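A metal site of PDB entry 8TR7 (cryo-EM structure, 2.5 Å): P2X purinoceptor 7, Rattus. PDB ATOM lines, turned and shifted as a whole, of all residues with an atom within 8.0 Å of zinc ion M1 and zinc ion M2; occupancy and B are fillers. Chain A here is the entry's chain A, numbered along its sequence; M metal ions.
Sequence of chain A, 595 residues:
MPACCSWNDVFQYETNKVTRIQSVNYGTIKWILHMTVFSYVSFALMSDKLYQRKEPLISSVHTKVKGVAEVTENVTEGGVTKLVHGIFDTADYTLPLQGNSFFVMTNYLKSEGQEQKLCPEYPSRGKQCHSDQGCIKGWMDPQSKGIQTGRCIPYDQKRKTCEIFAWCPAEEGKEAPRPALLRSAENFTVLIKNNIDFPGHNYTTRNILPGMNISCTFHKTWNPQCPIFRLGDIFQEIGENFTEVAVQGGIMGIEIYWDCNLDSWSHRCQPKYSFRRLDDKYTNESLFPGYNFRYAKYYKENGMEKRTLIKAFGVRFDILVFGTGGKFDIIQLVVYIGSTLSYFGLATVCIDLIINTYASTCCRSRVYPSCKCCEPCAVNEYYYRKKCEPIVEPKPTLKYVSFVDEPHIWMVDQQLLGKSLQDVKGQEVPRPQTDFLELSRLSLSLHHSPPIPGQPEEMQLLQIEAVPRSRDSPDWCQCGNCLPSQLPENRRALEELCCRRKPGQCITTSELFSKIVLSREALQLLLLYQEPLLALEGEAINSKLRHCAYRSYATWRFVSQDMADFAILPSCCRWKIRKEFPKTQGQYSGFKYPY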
ATOM      1  N   VAL A 404       4.823 -32.546   6.954  1.00  0.00           N
ATOM      2  CA  VAL A 404       4.343 -33.631   7.797  1.00  0.00           C
ATOM      3  C   VAL A 404       3.389 -34.536   7.017  1.00  0.00           C
ATOM      4  O   VAL A 404       3.362 -35.754   7.213  1.00  0.00           O
ATOM      5  CB  VAL A 404       3.683 -33.058   9.067  1.00  0.00           C
ATOM      6  CG1 VAL A 404       2.395 -32.360   8.722  1.00  0.00           C
ATOM      7  CG2 VAL A 404       3.451 -34.158  10.080  1.00  0.00           C
ATOM      8  N   GLN A 422       7.695 -22.077   0.014  1.00  0.00           N
ATOM      9  CA  GLN A 422       6.591 -23.024  -0.015  1.00  0.00           C
ATOM     10  C   GLN A 422       6.184 -23.349  -1.446  1.00  0.00           C
ATOM     11  O   GLN A 422       5.932 -24.520  -1.780  1.00  0.00           O
ATOM     12  CB  GLN A 422       5.405 -22.454   0.758  1.00  0.00           C
ATOM     13  CG  GLN A 422       4.222 -23.387   0.921  1.00  0.00           C
ATOM     14  CD  GLN A 422       4.298 -24.256   2.153  1.00  0.00           C
ATOM     15  OE1 GLN A 422       4.835 -23.861   3.184  1.00  0.00           O
ATOM     16  NE2 GLN A 422       3.732 -25.455   2.055  1.00  0.00           N
ATOM     17  N   SER A 473      -3.992 -15.076   8.525  1.00  0.00           N
ATOM     18  CA  SER A 473      -2.745 -15.791   8.355  1.00  0.00           C
ATOM     19  C   SER A 473      -2.294 -15.725   6.897  1.00  0.00           C
ATOM     20  O   SER A 473      -3.091 -15.485   5.999  1.00  0.00           O
ATOM     21  CB  SER A 473      -2.911 -17.249   8.785  1.00  0.00           C
ATOM     22  OG  SER A 473      -3.377 -18.055   7.711  1.00  0.00           O
ATOM     23  N   PRO A 474      -0.996 -15.936   6.653  1.00  0.00           N
ATOM     24  CA  PRO A 474      -0.500 -15.825   5.273  1.00  0.00           C
ATOM     25  C   PRO A 474      -1.175 -16.835   4.359  1.00  0.00           C
ATOM     26  O   PRO A 474      -1.576 -17.922   4.777  1.00  0.00           O
ATOM     27  CB  PRO A 474       0.996 -16.112   5.415  1.00  0.00           C
ATOM     28  CG  PRO A 474       1.309 -15.909   6.849  1.00  0.00           C
ATOM     29  CD  PRO A 474       0.078 -16.252   7.602  1.00  0.00           C
ATOM     30  N   TRP A 476       0.120 -18.576   1.892  1.00  0.00           N
ATOM     31  CA  TRP A 476       0.898 -19.788   1.724  1.00  0.00           C
ATOM     32  C   TRP A 476       0.763 -20.730   2.909  1.00  0.00           C
ATOM     33  O   TRP A 476       1.014 -21.930   2.766  1.00  0.00           O
ATOM     34  CB  TRP A 476       2.380 -19.447   1.501  1.00  0.00           C
ATOM     35  CG  TRP A 476       2.978 -18.505   2.496  1.00  0.00           C
ATOM     36  CD1 TRP A 476       3.216 -17.172   2.313  1.00  0.00           C
ATOM     37  CD2 TRP A 476       3.427 -18.808   3.815  1.00  0.00           C
ATOM     38  NE1 TRP A 476       3.781 -16.633   3.440  1.00  0.00           N
ATOM     39  CE2 TRP A 476       3.920 -17.615   4.385  1.00  0.00           C
ATOM     40  CE3 TRP A 476       3.461 -19.984   4.576  1.00  0.00           C
ATOM     41  CZ2 TRP A 476       4.433 -17.569   5.671  1.00  0.00           C
ATOM     42  CZ3 TRP A 476       3.966 -19.930   5.855  1.00  0.00           C
ATOM     43  CH2 TRP A 476       4.453 -18.725   6.392  1.00  0.00           C
ATOM     44  N   CYS A 477       0.362 -20.225   4.075  1.00  0.00           N
ATOM     45  CA  CYS A 477       0.170 -21.061   5.245  1.00  0.00           C
ATOM     46  C   CYS A 477      -1.229 -21.644   5.274  1.00  0.00           C
ATOM     47  O   CYS A 477      -2.190 -21.037   4.791  1.00  0.00           O
ATOM     48  CB  CYS A 477       0.411 -20.270   6.532  1.00  0.00           C
ATOM     49  SG  CYS A 477      -0.138 -21.132   8.033  1.00  0.00           S
ATOM     50  N   GLN A 478      -1.335 -22.839   5.852  1.00  0.00           N
ATOM     51  CA  GLN A 478      -2.624 -23.474   6.080  1.00  0.00           C
ATOM     52  C   GLN A 478      -2.710 -24.182   7.422  1.00  0.00           C
ATOM     53  O   GLN A 478      -3.712 -24.854   7.688  1.00  0.00           O
ATOM     54  CB  GLN A 478      -2.944 -24.465   4.964  1.00  0.00           C
ATOM     55  CG  GLN A 478      -1.781 -25.351   4.608  1.00  0.00           C
ATOM     56  CD  GLN A 478      -1.003 -24.819   3.428  1.00  0.00           C
ATOM     57  OE1 GLN A 478      -1.097 -23.642   3.082  1.00  0.00           O
ATOM     58  NE2 GLN A 478      -0.233 -25.691   2.789  1.00  0.00           N
ATOM     59  N   CYS A 479      -1.693 -24.061   8.279  1.00  0.00           N
ATOM     60  CA  CYS A 479      -1.730 -24.666   9.601  1.00  0.00           C
ATOM     61  C   CYS A 479      -2.282 -23.714  10.662  1.00  0.00           C
ATOM     62  O   CYS A 479      -2.469 -24.141  11.806  1.00  0.00           O
ATOM     63  CB  CYS A 479      -0.331 -25.132   9.999  1.00  0.00           C
ATOM     64  SG  CYS A 479       0.797 -23.839  10.580  1.00  0.00           S
ATOM     65  N   GLY A 480      -2.554 -22.462  10.304  1.00  0.00           N
ATOM     66  CA  GLY A 480      -3.154 -21.530  11.229  1.00  0.00           C
ATOM     67  C   GLY A 480      -2.245 -20.996  12.304  1.00  0.00           C
ATOM     68  O   GLY A 480      -2.727 -20.369  13.253  1.00  0.00           O
ATOM     69  N   ASN A 481      -0.935 -21.214  12.186  1.00  0.00           N
ATOM     70  CA  ASN A 481       0.014 -20.793  13.212  1.00  0.00           C
ATOM     71  C   ASN A 481       1.192 -19.989  12.685  1.00  0.00           C
ATOM     72  O   ASN A 481       1.845 -19.313  13.481  1.00  0.00           O
ATOM     73  CB  ASN A 481       0.551 -22.020  13.963  1.00  0.00           C
ATOM     74  CG  ASN A 481      -0.539 -22.853  14.589  1.00  0.00           C
ATOM     75  OD1 ASN A 481      -0.810 -23.973  14.140  1.00  0.00           O
ATOM     76  ND2 ASN A 481      -1.176 -22.322  15.616  1.00  0.00           N
ATOM     77  N   CYS A 482       1.472 -20.031  11.385  1.00  0.00           N
ATOM     78  CA  CYS A 482       2.608 -19.307  10.843  1.00  0.00           C
ATOM     79  C   CYS A 482       2.354 -17.805  10.872  1.00  0.00           C
ATOM     80  O   CYS A 482       1.209 -17.340  10.928  1.00  0.00           O
ATOM     81  CB  CYS A 482       2.889 -19.757   9.419  1.00  0.00           C
ATOM     82  SG  CYS A 482       3.449 -21.461   9.271  1.00  0.00           S
ATOM     83  N   LEU A 483       3.439 -17.038  10.858  1.00  0.00           N
ATOM     84  CA  LEU A 483       3.398 -15.584  10.908  1.00  0.00           C
ATOM     85  C   LEU A 483       4.289 -15.017   9.821  1.00  0.00           C
ATOM     86  O   LEU A 483       5.214 -15.677   9.339  1.00  0.00           O
ATOM     87  CB  LEU A 483       3.865 -15.074  12.272  1.00  0.00           C
ATOM     88  CG  LEU A 483       3.100 -15.569  13.507  1.00  0.00           C
ATOM     89  CD1 LEU A 483       3.730 -15.030  14.774  1.00  0.00           C
ATOM     90  CD2 LEU A 483       1.632 -15.189  13.431  1.00  0.00           C
ATOM     91  N   LEU A 497       7.696 -20.397   4.898  1.00  0.00           N
ATOM     92  CA  LEU A 497       7.477 -21.819   4.703  1.00  0.00           C
ATOM     93  C   LEU A 497       6.542 -22.336   5.798  1.00  0.00           C
ATOM     94  O   LEU A 497       6.614 -21.888   6.944  1.00  0.00           O
ATOM     95  CB  LEU A 497       8.799 -22.588   4.730  1.00  0.00           C
ATOM     96  CG  LEU A 497       8.746 -24.102   4.605  1.00  0.00           C
ATOM     97  CD1 LEU A 497       8.595 -24.552   3.167  1.00  0.00           C
ATOM     98  CD2 LEU A 497       9.988 -24.672   5.210  1.00  0.00           C
ATOM     99  N   CYS A 498       5.680 -23.269   5.428  1.00  0.00           N
ATOM    100  CA  CYS A 498       4.746 -23.893   6.353  1.00  0.00           C
ATOM    101  C   CYS A 498       5.175 -25.324   6.650  1.00  0.00           C
ATOM    102  O   CYS A 498       6.131 -25.861   6.076  1.00  0.00           O
ATOM    103  CB  CYS A 498       3.329 -23.879   5.787  1.00  0.00           C
ATOM    104  SG  CYS A 498       2.029 -24.112   7.015  1.00  0.00           S
ATOM    105  N   CYS A 499       4.431 -25.948   7.555  1.00  0.00           N
ATOM    106  CA  CYS A 499       4.674 -27.309   7.976  1.00  0.00           C
ATOM    107  C   CYS A 499       3.998 -28.353   7.094  1.00  0.00           C
ATOM    108  O   CYS A 499       4.235 -29.549   7.285  1.00  0.00           O
ATOM    109  CB  CYS A 499       4.220 -27.481   9.427  1.00  0.00           C
ATOM    110  SG  CYS A 499       2.467 -27.196   9.712  1.00  0.00           S
ATOM    111  N   ARG A 500       3.181 -27.947   6.122  1.00  0.00           N
ATOM    112  CA  ARG A 500       2.503 -28.893   5.257  1.00  0.00           C
ATOM    113  C   ARG A 500       2.083 -28.217   3.963  1.00  0.00           C
ATOM    114  O   ARG A 500       1.943 -27.001   3.894  1.00  0.00           O
ATOM    115  CB  ARG A 500       1.285 -29.509   5.959  1.00  0.00           C
ATOM    116  CG  ARG A 500       0.375 -28.490   6.613  1.00  0.00           C
ATOM    117  CD  ARG A 500      -0.679 -29.171   7.481  1.00  0.00           C
ATOM    118  NE  ARG A 500      -1.168 -30.403   6.884  1.00  0.00           N
ATOM    119  CZ  ARG A 500      -1.629 -31.442   7.579  1.00  0.00           C
ATOM    120  NH1 ARG A 500      -1.676 -31.416   8.896  1.00  0.00           N
ATOM    121  NH2 ARG A 500      -2.047 -32.515   6.929  1.00  0.00           N
ATOM    122  N   GLY A 504      -4.602 -28.674   7.255  1.00  0.00           N
ATOM    123  CA  GLY A 504      -4.672 -29.695   8.276  1.00  0.00           C
ATOM    124  C   GLY A 504      -4.157 -29.152   9.594  1.00  0.00           C
ATOM    125  O   GLY A 504      -3.980 -27.945   9.774  1.00  0.00           O
ATOM    126  N   GLN A 505      -3.917 -30.079  10.517  1.00  0.00           N
ATOM    127  CA  GLN A 505      -3.413 -29.723  11.837  1.00  0.00           C
ATOM    128  C   GLN A 505      -1.913 -29.499  11.791  1.00  0.00           C
ATOM    129  O   GLN A 505      -1.180 -30.219  11.108  1.00  0.00           O
ATOM    130  CB  GLN A 505      -3.753 -30.810  12.854  1.00  0.00           C
ATOM    131  CG  GLN A 505      -3.363 -32.211  12.422  1.00  0.00           C
ATOM    132  CD  GLN A 505      -3.461 -33.218  13.546  1.00  0.00           C
ATOM    133  OE1 GLN A 505      -3.410 -32.858  14.720  1.00  0.00           O
ATOM    134  NE2 GLN A 505      -3.604 -34.489  13.188  1.00  0.00           N
ATOM    135  N   CYS A 506      -1.457 -28.490  12.536  1.00  0.00           N
ATOM    136  CA  CYS A 506      -0.039 -28.175  12.587  1.00  0.00           C
ATOM    137  C   CYS A 506       0.732 -29.296  13.269  1.00  0.00           C
ATOM    138  O   CYS A 506       0.234 -29.971  14.170  1.00  0.00           O
ATOM    139  CB  CYS A 506       0.184 -26.871  13.348  1.00  0.00           C
ATOM    140  SG  CYS A 506       1.866 -26.247  13.262  1.00  0.00           S
ATOM    141  N   ILE A 507       1.976 -29.495  12.814  1.00  0.00           N
ATOM    142  CA  ILE A 507       2.841 -30.487  13.440  1.00  0.00           C
ATOM    143  C   ILE A 507       3.086 -30.139  14.894  1.00  0.00           C
ATOM    144  O   ILE A 507       3.192 -31.035  15.744  1.00  0.00           O
ATOM    145  CB  ILE A 507       4.168 -30.600  12.661  1.00  0.00           C
ATOM    146  CG1 ILE A 507       4.982 -31.784  13.169  1.00  0.00           C
ATOM    147  CG2 ILE A 507       4.975 -29.323  12.816  1.00  0.00           C
ATOM    148  CD1 ILE A 507       6.147 -32.135  12.286  1.00  0.00           C
ATOM    149  N   THR A 508       3.178 -28.852  15.210  1.00  0.00           N
ATOM    150  CA  THR A 508       3.503 -28.422  16.556  1.00  0.00           C
ATOM    151  C   THR A 508       2.411 -28.779  17.561  1.00  0.00           C
ATOM    152  O   THR A 508       2.661 -28.724  18.770  1.00  0.00           O
ATOM    153  CB  THR A 508       3.751 -26.915  16.590  1.00  0.00           C
ATOM    154  OG1 THR A 508       2.506 -26.225  16.434  1.00  0.00           O
ATOM    155  CG2 THR A 508       4.681 -26.485  15.484  1.00  0.00           C
ATOM    156  N   THR A 509       1.212 -29.124  17.095  1.00  0.00           N
ATOM    157  CA  THR A 509       0.153 -29.498  18.026  1.00  0.00           C
ATOM    158  C   THR A 509       0.472 -30.810  18.727  1.00  0.00           C
ATOM    159  O   THR A 509      -0.061 -31.075  19.814  1.00  0.00           O
ATOM    160  CB  THR A 509      -1.170 -29.618  17.277  1.00  0.00           C
ATOM    161  OG1 THR A 509      -1.012 -30.434  16.114  1.00  0.00           O
ATOM    162  CG2 THR A 509      -1.664 -28.235  16.862  1.00  0.00           C
ATOM    163  N   TYR A 553      14.555 -29.914  16.263  1.00  0.00           N
ATOM    164  CA  TYR A 553      13.564 -30.071  15.191  1.00  0.00           C
ATOM    165  C   TYR A 553      14.219 -30.562  13.913  1.00  0.00           C
ATOM    166  O   TYR A 553      13.709 -31.464  13.235  1.00  0.00           O
ATOM    167  CB  TYR A 553      12.827 -28.757  14.947  1.00  0.00           C
ATOM    168  CG  TYR A 553      11.881 -28.844  13.767  1.00  0.00           C
ATOM    169  CD1 TYR A 553      10.566 -29.246  13.941  1.00  0.00           C
ATOM    170  CD2 TYR A 553      12.312 -28.545  12.492  1.00  0.00           C
ATOM    171  CE1 TYR A 553       9.716 -29.336  12.875  1.00  0.00           C
ATOM    172  CE2 TYR A 553      11.468 -28.636  11.418  1.00  0.00           C
ATOM    173  CZ  TYR A 553      10.163 -29.032  11.611  1.00  0.00           C
ATOM    174  OH  TYR A 553       9.319 -29.124  10.537  1.00  0.00           O
ATOM    175  N   PRO A 570       9.856 -24.480   9.543  1.00  0.00           N
ATOM    176  CA  PRO A 570       8.607 -23.781   9.267  1.00  0.00           C
ATOM    177  C   PRO A 570       8.443 -22.555  10.139  1.00  0.00           C
ATOM    178  O   PRO A 570       8.971 -22.480  11.253  1.00  0.00           O
ATOM    179  CB  PRO A 570       7.533 -24.828   9.551  1.00  0.00           C
ATOM    180  CG  PRO A 570       8.224 -26.125   9.448  1.00  0.00           C
ATOM    181  CD  PRO A 570       9.625 -25.894   9.889  1.00  0.00           C
ATOM    182  N   SER A 571       7.703 -21.573   9.625  1.00  0.00           N
ATOM    183  CA  SER A 571       7.490 -20.343  10.369  1.00  0.00           C
ATOM    184  C   SER A 571       6.769 -20.607  11.682  1.00  0.00           C
ATOM    185  O   SER A 571       7.097 -20.020  12.717  1.00  0.00           O
ATOM    186  CB  SER A 571       6.706 -19.354   9.511  1.00  0.00           C
ATOM    187  OG  SER A 571       6.448 -18.157  10.226  1.00  0.00           O
ATOM    188  N   CYS A 572       5.773 -21.496  11.674  1.00  0.00           N
ATOM    189  CA  CYS A 572       5.040 -21.819  12.886  1.00  0.00           C
ATOM    190  C   CYS A 572       5.986 -22.316  13.977  1.00  0.00           C
ATOM    191  O   CYS A 572       6.007 -21.787  15.093  1.00  0.00           O
ATOM    192  CB  CYS A 572       3.956 -22.848  12.581  1.00  0.00           C
ATOM    193  SG  CYS A 572       4.477 -24.282  11.593  1.00  0.00           S
ATOM    194  N   CYS A 573       6.787 -23.331  13.648  1.00  0.00           N
ATOM    195  CA  CYS A 573       7.700 -23.913  14.626  1.00  0.00           C
ATOM    196  C   CYS A 573       8.749 -22.901  15.074  1.00  0.00           C
ATOM    197  O   CYS A 573       9.060 -22.803  16.270  1.00  0.00           O
ATOM    198  CB  CYS A 573       8.355 -25.139  14.021  1.00  0.00           C
ATOM    199  SG  CYS A 573       7.199 -26.227  13.172  1.00  0.00           S
ATOM    200  N   LYS A 576       7.118 -20.286  17.350  1.00  0.00           N
ATOM    201  CA  LYS A 576       6.789 -20.917  18.631  1.00  0.00           C
ATOM    202  C   LYS A 576       8.035 -21.076  19.490  1.00  0.00           C
ATOM    203  O   LYS A 576       8.020 -20.758  20.684  1.00  0.00           O
ATOM    204  CB  LYS A 576       6.142 -22.260  18.369  1.00  0.00           C
ATOM    205  CG  LYS A 576       5.616 -22.964  19.600  1.00  0.00           C
ATOM    206  CD  LYS A 576       4.988 -24.291  19.235  1.00  0.00           C
ATOM    207  CE  LYS A 576       3.673 -24.116  18.499  1.00  0.00           C
ATOM    208  NZ  LYS A 576       2.595 -23.522  19.325  1.00  0.00           N
HETATM  209 ZN    ZN M   1       1.512 -22.619   8.726  1.00  0.00          ZN
HETATM  210 ZN    ZN M   2       2.443 -25.369  11.190  1.00  0.00          ZN
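Of the 28 residues printed, 4 come within 4 Å of zinc ion M1.
SG of Cys 506 lies close to OD1 of Asn 481 (3.6 Å). OG1 of Thr 508 lies close to SG of Cys 506 (3.2 Å). The backbone NH (N) of Gly 480 sits close to the side-chain sulfur (SG) of Cys 477 (3.6 Å). SG of Cys 498 sits close to N of Gln 478, at 3.8 Å. The side-chain amide oxygen (OE1) of Gln 422 sits at hydrogen-bond distance from the backbone NH (N) of Cys 498, at 2.5 Å. The backbone carbonyl oxygen (O) of Cys 479 sits close to the side-chain amide oxygen (OD1) of Asn 481, 2.9 Å away. The side-chain sulfur (SG) of Cys 573 lies close to the side-chain sulfur (SG) of Cys 572 (3.7 Å). O of Cys 499 is in hydrogen-bond range of N of Val 404 (3.1 Å).
Zinc ion M2 is bound by SG of Cys 506 (2.3 Å), SG of Cys 479 (2.3 Å), SG of Cys 572 (2.3 Å) and SG of Cys 499 (2.4 Å).
Of the 28 residues printed, 4 come within 4 Å of zinc ion M2. Along chain A the residues within 4 Å of zinc ion M2 span positions 479 to 572. The nearest printed residue that does not touch zinc ion M2 is Cys 498 (4.4 Å).
SG of Cys 482 binds zinc ion M1 (2.3 Å). Zinc ion M1 is bound by SG of Cys 477 (2.3 Å). SG of Cys 498 is bound to zinc ion M1 (2.3 Å). Zinc ion M1 is bound by the side-chain sulfur (SG) of Cys 479 (2.3 Å). Zinc ion M1 has four donor atoms within binding distance.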
